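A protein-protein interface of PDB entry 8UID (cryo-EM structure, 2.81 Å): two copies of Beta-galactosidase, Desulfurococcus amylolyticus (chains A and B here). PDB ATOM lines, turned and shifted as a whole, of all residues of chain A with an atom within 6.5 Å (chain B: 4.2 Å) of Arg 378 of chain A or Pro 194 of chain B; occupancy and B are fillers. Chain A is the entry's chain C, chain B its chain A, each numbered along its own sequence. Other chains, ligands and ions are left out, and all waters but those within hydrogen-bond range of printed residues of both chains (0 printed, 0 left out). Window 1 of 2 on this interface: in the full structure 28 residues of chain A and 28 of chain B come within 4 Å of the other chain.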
ATOM      1  N   TRP A 195       8.162 -10.380  35.014  1.00  0.00           N
ATOM      2  CA  TRP A 195       8.814 -11.678  35.216  1.00  0.00           C
ATOM      3  C   TRP A 195       9.772 -11.760  36.416  1.00  0.00           C
ATOM      4  O   TRP A 195      10.304 -12.830  36.704  1.00  0.00           O
ATOM      5  CB  TRP A 195       9.326 -12.245  33.882  1.00  0.00           C
ATOM      6  CG  TRP A 195       8.373 -11.990  32.746  1.00  0.00           C
ATOM      7  CD1 TRP A 195       8.604 -11.200  31.676  1.00  0.00           C
ATOM      8  CD2 TRP A 195       6.970 -12.378  32.655  1.00  0.00           C
ATOM      9  NE1 TRP A 195       7.433 -11.032  30.963  1.00  0.00           N
ATOM     10  CE2 TRP A 195       6.379 -11.677  31.564  1.00  0.00           C
ATOM     11  CE3 TRP A 195       6.127 -13.189  33.437  1.00  0.00           C
ATOM     12  CZ2 TRP A 195       5.008 -11.734  31.297  1.00  0.00           C
ATOM     13  CZ3 TRP A 195       4.750 -13.259  33.171  1.00  0.00           C
ATOM     14  CH2 TRP A 195       4.191 -12.522  32.123  1.00  0.00           C
ATOM     15  N   GLU A 244      -0.522 -10.194  30.620  1.00  0.00           N
ATOM     16  CA  GLU A 244      -0.188 -11.495  31.197  1.00  0.00           C
ATOM     17  C   GLU A 244       0.414 -11.369  32.594  1.00  0.00           C
ATOM     18  O   GLU A 244       0.190 -12.220  33.448  1.00  0.00           O
ATOM     19  CB  GLU A 244       0.860 -12.216  30.327  1.00  0.00           C
ATOM     20  CG  GLU A 244       0.548 -12.365  28.836  1.00  0.00           C
ATOM     21  CD  GLU A 244       1.237 -11.287  27.990  1.00  0.00           C
ATOM     22  OE1 GLU A 244       2.034 -11.632  27.088  1.00  0.00           O
ATOM     23  OE2 GLU A 244       0.967 -10.094  28.228  1.00  0.00           O
ATOM     24  N   TRP A 245       1.187 -10.307  32.831  1.00  0.00           N
ATOM     25  CA  TRP A 245       1.896 -10.076  34.081  1.00  0.00           C
ATOM     26  C   TRP A 245       0.925  -9.766  35.206  1.00  0.00           C
ATOM     27  O   TRP A 245       0.902 -10.478  36.198  1.00  0.00           O
ATOM     28  CB  TRP A 245       2.945  -8.979  33.890  1.00  0.00           C
ATOM     29  CG  TRP A 245       3.740  -8.631  35.102  1.00  0.00           C
ATOM     30  CD1 TRP A 245       3.873  -7.407  35.653  1.00  0.00           C
ATOM     31  CD2 TRP A 245       4.574  -9.515  35.894  1.00  0.00           C
ATOM     32  NE1 TRP A 245       4.762  -7.465  36.704  1.00  0.00           N
ATOM     33  CE2 TRP A 245       5.231  -8.746  36.891  1.00  0.00           C
ATOM     34  CE3 TRP A 245       4.868 -10.886  35.830  1.00  0.00           C
ATOM     35  CZ2 TRP A 245       6.175  -9.317  37.748  1.00  0.00           C
ATOM     36  CZ3 TRP A 245       5.763 -11.473  36.730  1.00  0.00           C
ATOM     37  CH2 TRP A 245       6.418 -10.691  37.687  1.00  0.00           C
ATOM     38  N   ILE A 248      -0.828 -12.941  36.331  1.00  0.00           N
ATOM     39  CA  ILE A 248       0.067 -13.825  37.080  1.00  0.00           C
ATOM     40  C   ILE A 248       0.264 -13.324  38.504  1.00  0.00           C
ATOM     41  O   ILE A 248       0.331 -14.135  39.422  1.00  0.00           O
ATOM     42  CB  ILE A 248       1.407 -14.023  36.320  1.00  0.00           C
ATOM     43  CG1 ILE A 248       1.662 -15.526  36.165  1.00  0.00           C
ATOM     44  CG2 ILE A 248       2.628 -13.345  36.964  1.00  0.00           C
ATOM     45  CD1 ILE A 248       2.802 -15.874  35.211  1.00  0.00           C
ATOM     46  N   ARG A 302      -8.509 -10.274  31.366  1.00  0.00           N
ATOM     47  CA  ARG A 302      -7.682 -11.109  32.237  1.00  0.00           C
ATOM     48  C   ARG A 302      -8.015 -10.924  33.708  1.00  0.00           C
ATOM     49  O   ARG A 302      -8.334 -11.892  34.382  1.00  0.00           O
ATOM     50  CB  ARG A 302      -6.212 -10.814  31.972  1.00  0.00           C
ATOM     51  CG  ARG A 302      -5.760 -11.385  30.633  1.00  0.00           C
ATOM     52  CD  ARG A 302      -4.247 -11.345  30.555  1.00  0.00           C
ATOM     53  NE  ARG A 302      -3.755 -12.129  29.416  1.00  0.00           N
ATOM     54  CZ  ARG A 302      -3.196 -13.315  29.463  1.00  0.00           C
ATOM     55  NH1 ARG A 302      -3.157 -14.029  30.548  1.00  0.00           N
ATOM     56  NH2 ARG A 302      -2.647 -13.802  28.396  1.00  0.00           N
ATOM     57  N   ASN A 350       3.438 -20.889  35.464  1.00  0.00           N
ATOM     58  CA  ASN A 350       4.403 -21.028  34.396  1.00  0.00           C
ATOM     59  C   ASN A 350       4.865 -19.629  33.989  1.00  0.00           C
ATOM     60  O   ASN A 350       4.225 -18.949  33.193  1.00  0.00           O
ATOM     61  CB  ASN A 350       3.737 -21.805  33.256  1.00  0.00           C
ATOM     62  CG  ASN A 350       4.648 -22.022  32.076  1.00  0.00           C
ATOM     63  OD1 ASN A 350       5.854 -21.881  32.154  1.00  0.00           O
ATOM     64  ND2 ASN A 350       4.096 -22.370  30.948  1.00  0.00           N
ATOM     65  N   THR A 351       5.976 -19.174  34.554  1.00  0.00           N
ATOM     66  CA  THR A 351       6.621 -17.910  34.166  1.00  0.00           C
ATOM     67  C   THR A 351       7.379 -17.993  32.831  1.00  0.00           C
ATOM     68  O   THR A 351       7.772 -16.960  32.287  1.00  0.00           O
ATOM     69  CB  THR A 351       7.560 -17.432  35.279  1.00  0.00           C
ATOM     70  OG1 THR A 351       8.444 -18.448  35.696  1.00  0.00           O
ATOM     71  CG2 THR A 351       6.799 -16.959  36.508  1.00  0.00           C
ATOM     72  N   GLY A 352       7.572 -19.191  32.274  1.00  0.00           N
ATOM     73  CA  GLY A 352       8.252 -19.412  30.997  1.00  0.00           C
ATOM     74  C   GLY A 352       7.379 -19.171  29.771  1.00  0.00           C
ATOM     75  O   GLY A 352       6.155 -19.183  29.848  1.00  0.00           O
ATOM     76  N   ASP A 353       8.004 -18.956  28.619  1.00  0.00           N
ATOM     77  CA  ASP A 353       7.319 -18.797  27.331  1.00  0.00           C
ATOM     78  C   ASP A 353       7.099 -20.124  26.577  1.00  0.00           C
ATOM     79  O   ASP A 353       6.523 -20.126  25.491  1.00  0.00           O
ATOM     80  CB  ASP A 353       8.006 -17.730  26.463  1.00  0.00           C
ATOM     81  CG  ASP A 353       9.425 -18.064  25.992  1.00  0.00           C
ATOM     82  OD1 ASP A 353      10.034 -19.039  26.475  1.00  0.00           O
ATOM     83  OD2 ASP A 353       9.946 -17.327  25.127  1.00  0.00           O
ATOM     84  N   ASN A 354       7.493 -21.263  27.149  1.00  0.00           N
ATOM     85  CA  ASN A 354       7.065 -22.589  26.705  1.00  0.00           C
ATOM     86  C   ASN A 354       5.717 -22.990  27.313  1.00  0.00           C
ATOM     87  O   ASN A 354       5.388 -22.629  28.440  1.00  0.00           O
ATOM     88  CB  ASN A 354       8.142 -23.626  27.049  1.00  0.00           C
ATOM     89  CG  ASN A 354       9.413 -23.439  26.246  1.00  0.00           C
ATOM     90  OD1 ASN A 354       9.396 -23.130  25.064  1.00  0.00           O
ATOM     91  ND2 ASN A 354      10.558 -23.630  26.850  1.00  0.00           N
ATOM     92  N   VAL A 375      -0.648 -25.971  31.258  1.00  0.00           N
ATOM     93  CA  VAL A 375      -0.392 -24.636  31.813  1.00  0.00           C
ATOM     94  C   VAL A 375       0.203 -23.760  30.706  1.00  0.00           C
ATOM     95  O   VAL A 375       1.368 -23.941  30.354  1.00  0.00           O
ATOM     96  CB  VAL A 375       0.508 -24.678  33.061  1.00  0.00           C
ATOM     97  CG1 VAL A 375       0.538 -23.297  33.721  1.00  0.00           C
ATOM     98  CG2 VAL A 375       0.013 -25.679  34.105  1.00  0.00           C
ATOM     99  N   PRO A 376      -0.565 -22.821  30.128  1.00  0.00           N
ATOM    100  CA  PRO A 376      -0.107 -21.935  29.060  1.00  0.00           C
ATOM    101  C   PRO A 376       1.213 -21.201  29.354  1.00  0.00           C
ATOM    102  O   PRO A 376       1.582 -21.049  30.514  1.00  0.00           O
ATOM    103  CB  PRO A 376      -1.265 -20.975  28.818  1.00  0.00           C
ATOM    104  CG  PRO A 376      -2.476 -21.839  29.136  1.00  0.00           C
ATOM    105  CD  PRO A 376      -1.997 -22.660  30.318  1.00  0.00           C
ATOM    106  N   PRO A 377       1.957 -20.737  28.343  1.00  0.00           N
ATOM    107  CA  PRO A 377       3.113 -19.878  28.563  1.00  0.00           C
ATOM    108  C   PRO A 377       2.721 -18.536  29.185  1.00  0.00           C
ATOM    109  O   PRO A 377       1.661 -17.996  28.870  1.00  0.00           O
ATOM    110  CB  PRO A 377       3.726 -19.703  27.179  1.00  0.00           C
ATOM    111  CG  PRO A 377       2.573 -19.919  26.214  1.00  0.00           C
ATOM    112  CD  PRO A 377       1.737 -20.964  26.929  1.00  0.00           C
ATOM    113  N   ARG A 378       3.581 -17.963  30.037  1.00  0.00           N
ATOM    114  CA  ARG A 378       3.347 -16.682  30.739  1.00  0.00           C
ATOM    115  C   ARG A 378       1.989 -16.684  31.460  1.00  0.00           C
ATOM    116  O   ARG A 378       1.134 -15.836  31.228  1.00  0.00           O
ATOM    117  CB  ARG A 378       3.549 -15.490  29.768  1.00  0.00           C
ATOM    118  CG  ARG A 378       4.948 -14.883  29.832  1.00  0.00           C
ATOM    119  CD  ARG A 378       6.049 -15.716  29.199  1.00  0.00           C
ATOM    120  NE  ARG A 378       7.347 -15.412  29.824  1.00  0.00           N
ATOM    121  CZ  ARG A 378       8.318 -14.661  29.350  1.00  0.00           C
ATOM    122  NH1 ARG A 378       8.206 -14.003  28.239  1.00  0.00           N
ATOM    123  NH2 ARG A 378       9.439 -14.577  29.992  1.00  0.00           N
ATOM    124  N   TYR A 379       1.748 -17.678  32.306  1.00  0.00           N
ATOM    125  CA  TYR A 379       0.418 -17.947  32.850  1.00  0.00           C
ATOM    126  C   TYR A 379       0.466 -18.534  34.252  1.00  0.00           C
ATOM    127  O   TYR A 379       1.441 -19.164  34.631  1.00  0.00           O
ATOM    128  CB  TYR A 379      -0.314 -18.897  31.901  1.00  0.00           C
ATOM    129  CG  TYR A 379      -1.817 -18.904  32.040  1.00  0.00           C
ATOM    130  CD1 TYR A 379      -2.577 -17.868  31.474  1.00  0.00           C
ATOM    131  CD2 TYR A 379      -2.452 -19.941  32.733  1.00  0.00           C
ATOM    132  CE1 TYR A 379      -3.973 -17.841  31.647  1.00  0.00           C
ATOM    133  CE2 TYR A 379      -3.846 -19.928  32.893  1.00  0.00           C
ATOM    134  CZ  TYR A 379      -4.603 -18.864  32.376  1.00  0.00           C
ATOM    135  OH  TYR A 379      -5.934 -18.823  32.620  1.00  0.00           O
ATOM    136  N   ALA A 380      -0.596 -18.388  35.029  1.00  0.00           N
ATOM    137  CA  ALA A 380      -0.814 -19.183  36.225  1.00  0.00           C
ATOM    138  C   ALA A 380      -2.203 -19.787  36.149  1.00  0.00           C
ATOM    139  O   ALA A 380      -3.157 -19.056  35.981  1.00  0.00           O
ATOM    140  CB  ALA A 380      -0.607 -18.319  37.472  1.00  0.00           C
ATOM    141  N   PRO B 192      16.392 -17.086  22.491  1.00  0.00           N
ATOM    142  CA  PRO B 192      16.240 -16.990  23.944  1.00  0.00           C
ATOM    143  C   PRO B 192      14.858 -16.468  24.367  1.00  0.00           C
ATOM    144  O   PRO B 192      14.307 -15.579  23.727  1.00  0.00           O
ATOM    145  CB  PRO B 192      17.340 -16.024  24.375  1.00  0.00           C
ATOM    146  CG  PRO B 192      17.387 -15.057  23.203  1.00  0.00           C
ATOM    147  CD  PRO B 192      17.224 -15.991  22.015  1.00  0.00           C
ATOM    148  N   SER B 193      14.320 -16.936  25.494  1.00  0.00           N
ATOM    149  CA  SER B 193      13.105 -16.350  26.080  1.00  0.00           C
ATOM    150  C   SER B 193      13.329 -14.888  26.496  1.00  0.00           C
ATOM    151  O   SER B 193      14.414 -14.567  26.980  1.00  0.00           O
ATOM    152  CB  SER B 193      12.643 -17.138  27.304  1.00  0.00           C
ATOM    153  OG  SER B 193      12.370 -18.478  26.935  1.00  0.00           O
ATOM    154  N   PRO B 194      12.333 -13.988  26.380  1.00  0.00           N
ATOM    155  CA  PRO B 194      12.523 -12.573  26.667  1.00  0.00           C
ATOM    156  C   PRO B 194      13.136 -12.260  28.033  1.00  0.00           C
ATOM    157  O   PRO B 194      12.735 -12.796  29.066  1.00  0.00           O
ATOM    158  CB  PRO B 194      11.174 -11.909  26.442  1.00  0.00           C
ATOM    159  CG  PRO B 194      10.572 -12.789  25.351  1.00  0.00           C
ATOM    160  CD  PRO B 194      11.051 -14.183  25.724  1.00  0.00           C
ATOM    161  N   TRP B 195      14.118 -11.362  28.010  1.00  0.00           N
ATOM    162  CA  TRP B 195      14.901 -10.863  29.144  1.00  0.00           C
ATOM    163  C   TRP B 195      15.890 -11.865  29.762  1.00  0.00           C
ATOM    164  O   TRP B 195      16.639 -11.506  30.667  1.00  0.00           O
ATOM    165  CB  TRP B 195      14.005 -10.082  30.123  1.00  0.00           C
ATOM    166  CG  TRP B 195      12.981  -9.236  29.415  1.00  0.00           C
ATOM    167  CD1 TRP B 195      11.643  -9.411  29.453  1.00  0.00           C
ATOM    168  CD2 TRP B 195      13.216  -8.199  28.417  1.00  0.00           C
ATOM    169  NE1 TRP B 195      11.044  -8.593  28.514  1.00  0.00           N
ATOM    170  CE2 TRP B 195      11.975  -7.879  27.798  1.00  0.00           C
ATOM    171  CE3 TRP B 195      14.370  -7.560  27.923  1.00  0.00           C
ATOM    172  CZ2 TRP B 195      11.887  -7.012  26.706  1.00  0.00           C
ATOM    173  CZ3 TRP B 195      14.291  -6.682  26.833  1.00  0.00           C
ATOM    174  CH2 TRP B 195      13.063  -6.424  26.214  1.00  0.00           C
ATOM    175  N   ASP B 196      16.009 -13.078  29.215  1.00  0.00           N
ATOM    176  CA  ASP B 196      17.104 -14.009  29.503  1.00  0.00           C
ATOM    177  C   ASP B 196      18.379 -13.661  28.701  1.00  0.00           C
ATOM    178  O   ASP B 196      18.797 -14.382  27.791  1.00  0.00           O
ATOM    179  CB  ASP B 196      16.621 -15.450  29.275  1.00  0.00           C
ATOM    180  CG  ASP B 196      17.578 -16.521  29.822  1.00  0.00           C
ATOM    181  OD1 ASP B 196      18.696 -16.200  30.286  1.00  0.00           O
ATOM    182  OD2 ASP B 196      17.166 -17.703  29.821  1.00  0.00           O
ATOM    183  N   LEU B 239       4.116 -16.510  24.211  1.00  0.00           N
ATOM    184  CA  LEU B 239       3.029 -16.329  23.252  1.00  0.00           C
ATOM    185  C   LEU B 239       3.314 -15.165  22.305  1.00  0.00           C
ATOM    186  O   LEU B 239       3.087 -15.281  21.115  1.00  0.00           O
ATOM    187  CB  LEU B 239       1.694 -16.070  23.978  1.00  0.00           C
ATOM    188  CG  LEU B 239       1.462 -16.834  25.291  1.00  0.00           C
ATOM    189  CD1 LEU B 239       1.910 -16.013  26.501  1.00  0.00           C
ATOM    190  CD2 LEU B 239      -0.020 -17.130  25.486  1.00  0.00           C
ATOM    191  N   PRO B 242       8.558  -9.711  22.419  1.00  0.00           N
ATOM    192  CA  PRO B 242       8.578  -8.255  22.413  1.00  0.00           C
ATOM    193  C   PRO B 242       9.412  -7.708  21.240  1.00  0.00           C
ATOM    194  O   PRO B 242      10.514  -8.206  21.000  1.00  0.00           O
ATOM    195  CB  PRO B 242       9.136  -7.855  23.779  1.00  0.00           C
ATOM    196  CG  PRO B 242       8.844  -9.060  24.660  1.00  0.00           C
ATOM    197  CD  PRO B 242       8.994 -10.224  23.700  1.00  0.00           C
ATOM    198  N   TRP B 245      12.785  -6.814  22.447  1.00  0.00           N
ATOM    199  CA  TRP B 245      13.679  -7.936  22.690  1.00  0.00           C
ATOM    200  C   TRP B 245      14.562  -8.198  21.485  1.00  0.00           C
ATOM    201  O   TRP B 245      15.778  -8.148  21.603  1.00  0.00           O
ATOM    202  CB  TRP B 245      12.868  -9.166  23.104  1.00  0.00           C
ATOM    203  CG  TRP B 245      13.663 -10.398  23.375  1.00  0.00           C
ATOM    204  CD1 TRP B 245      13.497 -11.604  22.794  1.00  0.00           C
ATOM    205  CD2 TRP B 245      14.723 -10.569  24.349  1.00  0.00           C
ATOM    206  NE1 TRP B 245      14.353 -12.517  23.370  1.00  0.00           N
ATOM    207  CE2 TRP B 245      15.130 -11.929  24.344  1.00  0.00           C
ATOM    208  CE3 TRP B 245      15.345  -9.707  25.267  1.00  0.00           C
ATOM    209  CZ2 TRP B 245      16.077 -12.412  25.250  1.00  0.00           C
ATOM    210  CZ3 TRP B 245      16.341 -10.170  26.130  1.00  0.00           C
ATOM    211  CH2 TRP B 245      16.708 -11.521  26.124  1.00  0.00           C
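The side-chain hydroxyl of Ser 193 of chain B is in hydrogen-bond range of the side-chain carboxylate of Asp 353 of chain A, 2.4 Å away.
The backbone carbonyl oxygen of Asn 350 of chain A is in hydrogen-bond range of the backbone NH of Arg 378 of chain A (3.4 Å). O of Thr 351 of chain A sits at hydrogen-bond distance from NE of Arg 378 of chain A. O of Gly 352 of chain A is in hydrogen-bond range of N of Arg 378 of chain A (2.9 Å).
Among the printed residues, pairs that only touch across the chains: Asp 353 of chain A with Pro 194 of chain B, Pro 377 of chain A with Leu 239 of chain B, Arg 378 of chain A with Pro 194 of chain B and Arg 378 of chain A with Leu 239 of chain B.
Printed residues of chain B within 4 Å of Asp 353 of chain A: Ser 193 and Pro 194. Val 375 of chain A touches none of the printed residues of chain B. Of the printed residues of chain B, Pro 377 of chain A touches Leu 239 (3.1 Å). Of chain B, only Pro 194 and Leu 239 come within 4 Å of Arg 378 of chain A. Pro 192 of chain B touches none of the printed residues of chain A. Of the printed residues of chain A, Ser 193 of chain B touches Asp 353 (2.4 Å). Pro 194 of chain B touches just these residues of chain A: Asp 353 (3.4 Å) and Arg 378 (3.8 Å). Of the printed residues of chain A, Leu 239 of chain B touches Pro 377 and Arg 378. The nearest residue of chain A that does not touch Pro 194 of chain B is Trp 195 of chain A (5.1 Å).
Hydrophobic or aromatic side chains of chain A that line the printed part of chain B: Pro 377. Printed residues of chain B that touch a printed residue of chain A: Ser 193, Pro 194 and Leu 239. Along chain B the printed residues that touch a printed residue of chain A span positions 193 to 239.
Positions printed for both chains: 195 and 245. Of the 5 pairs that touch across the chains among the printed residues, none has its exchanged pair printed and touching as well.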
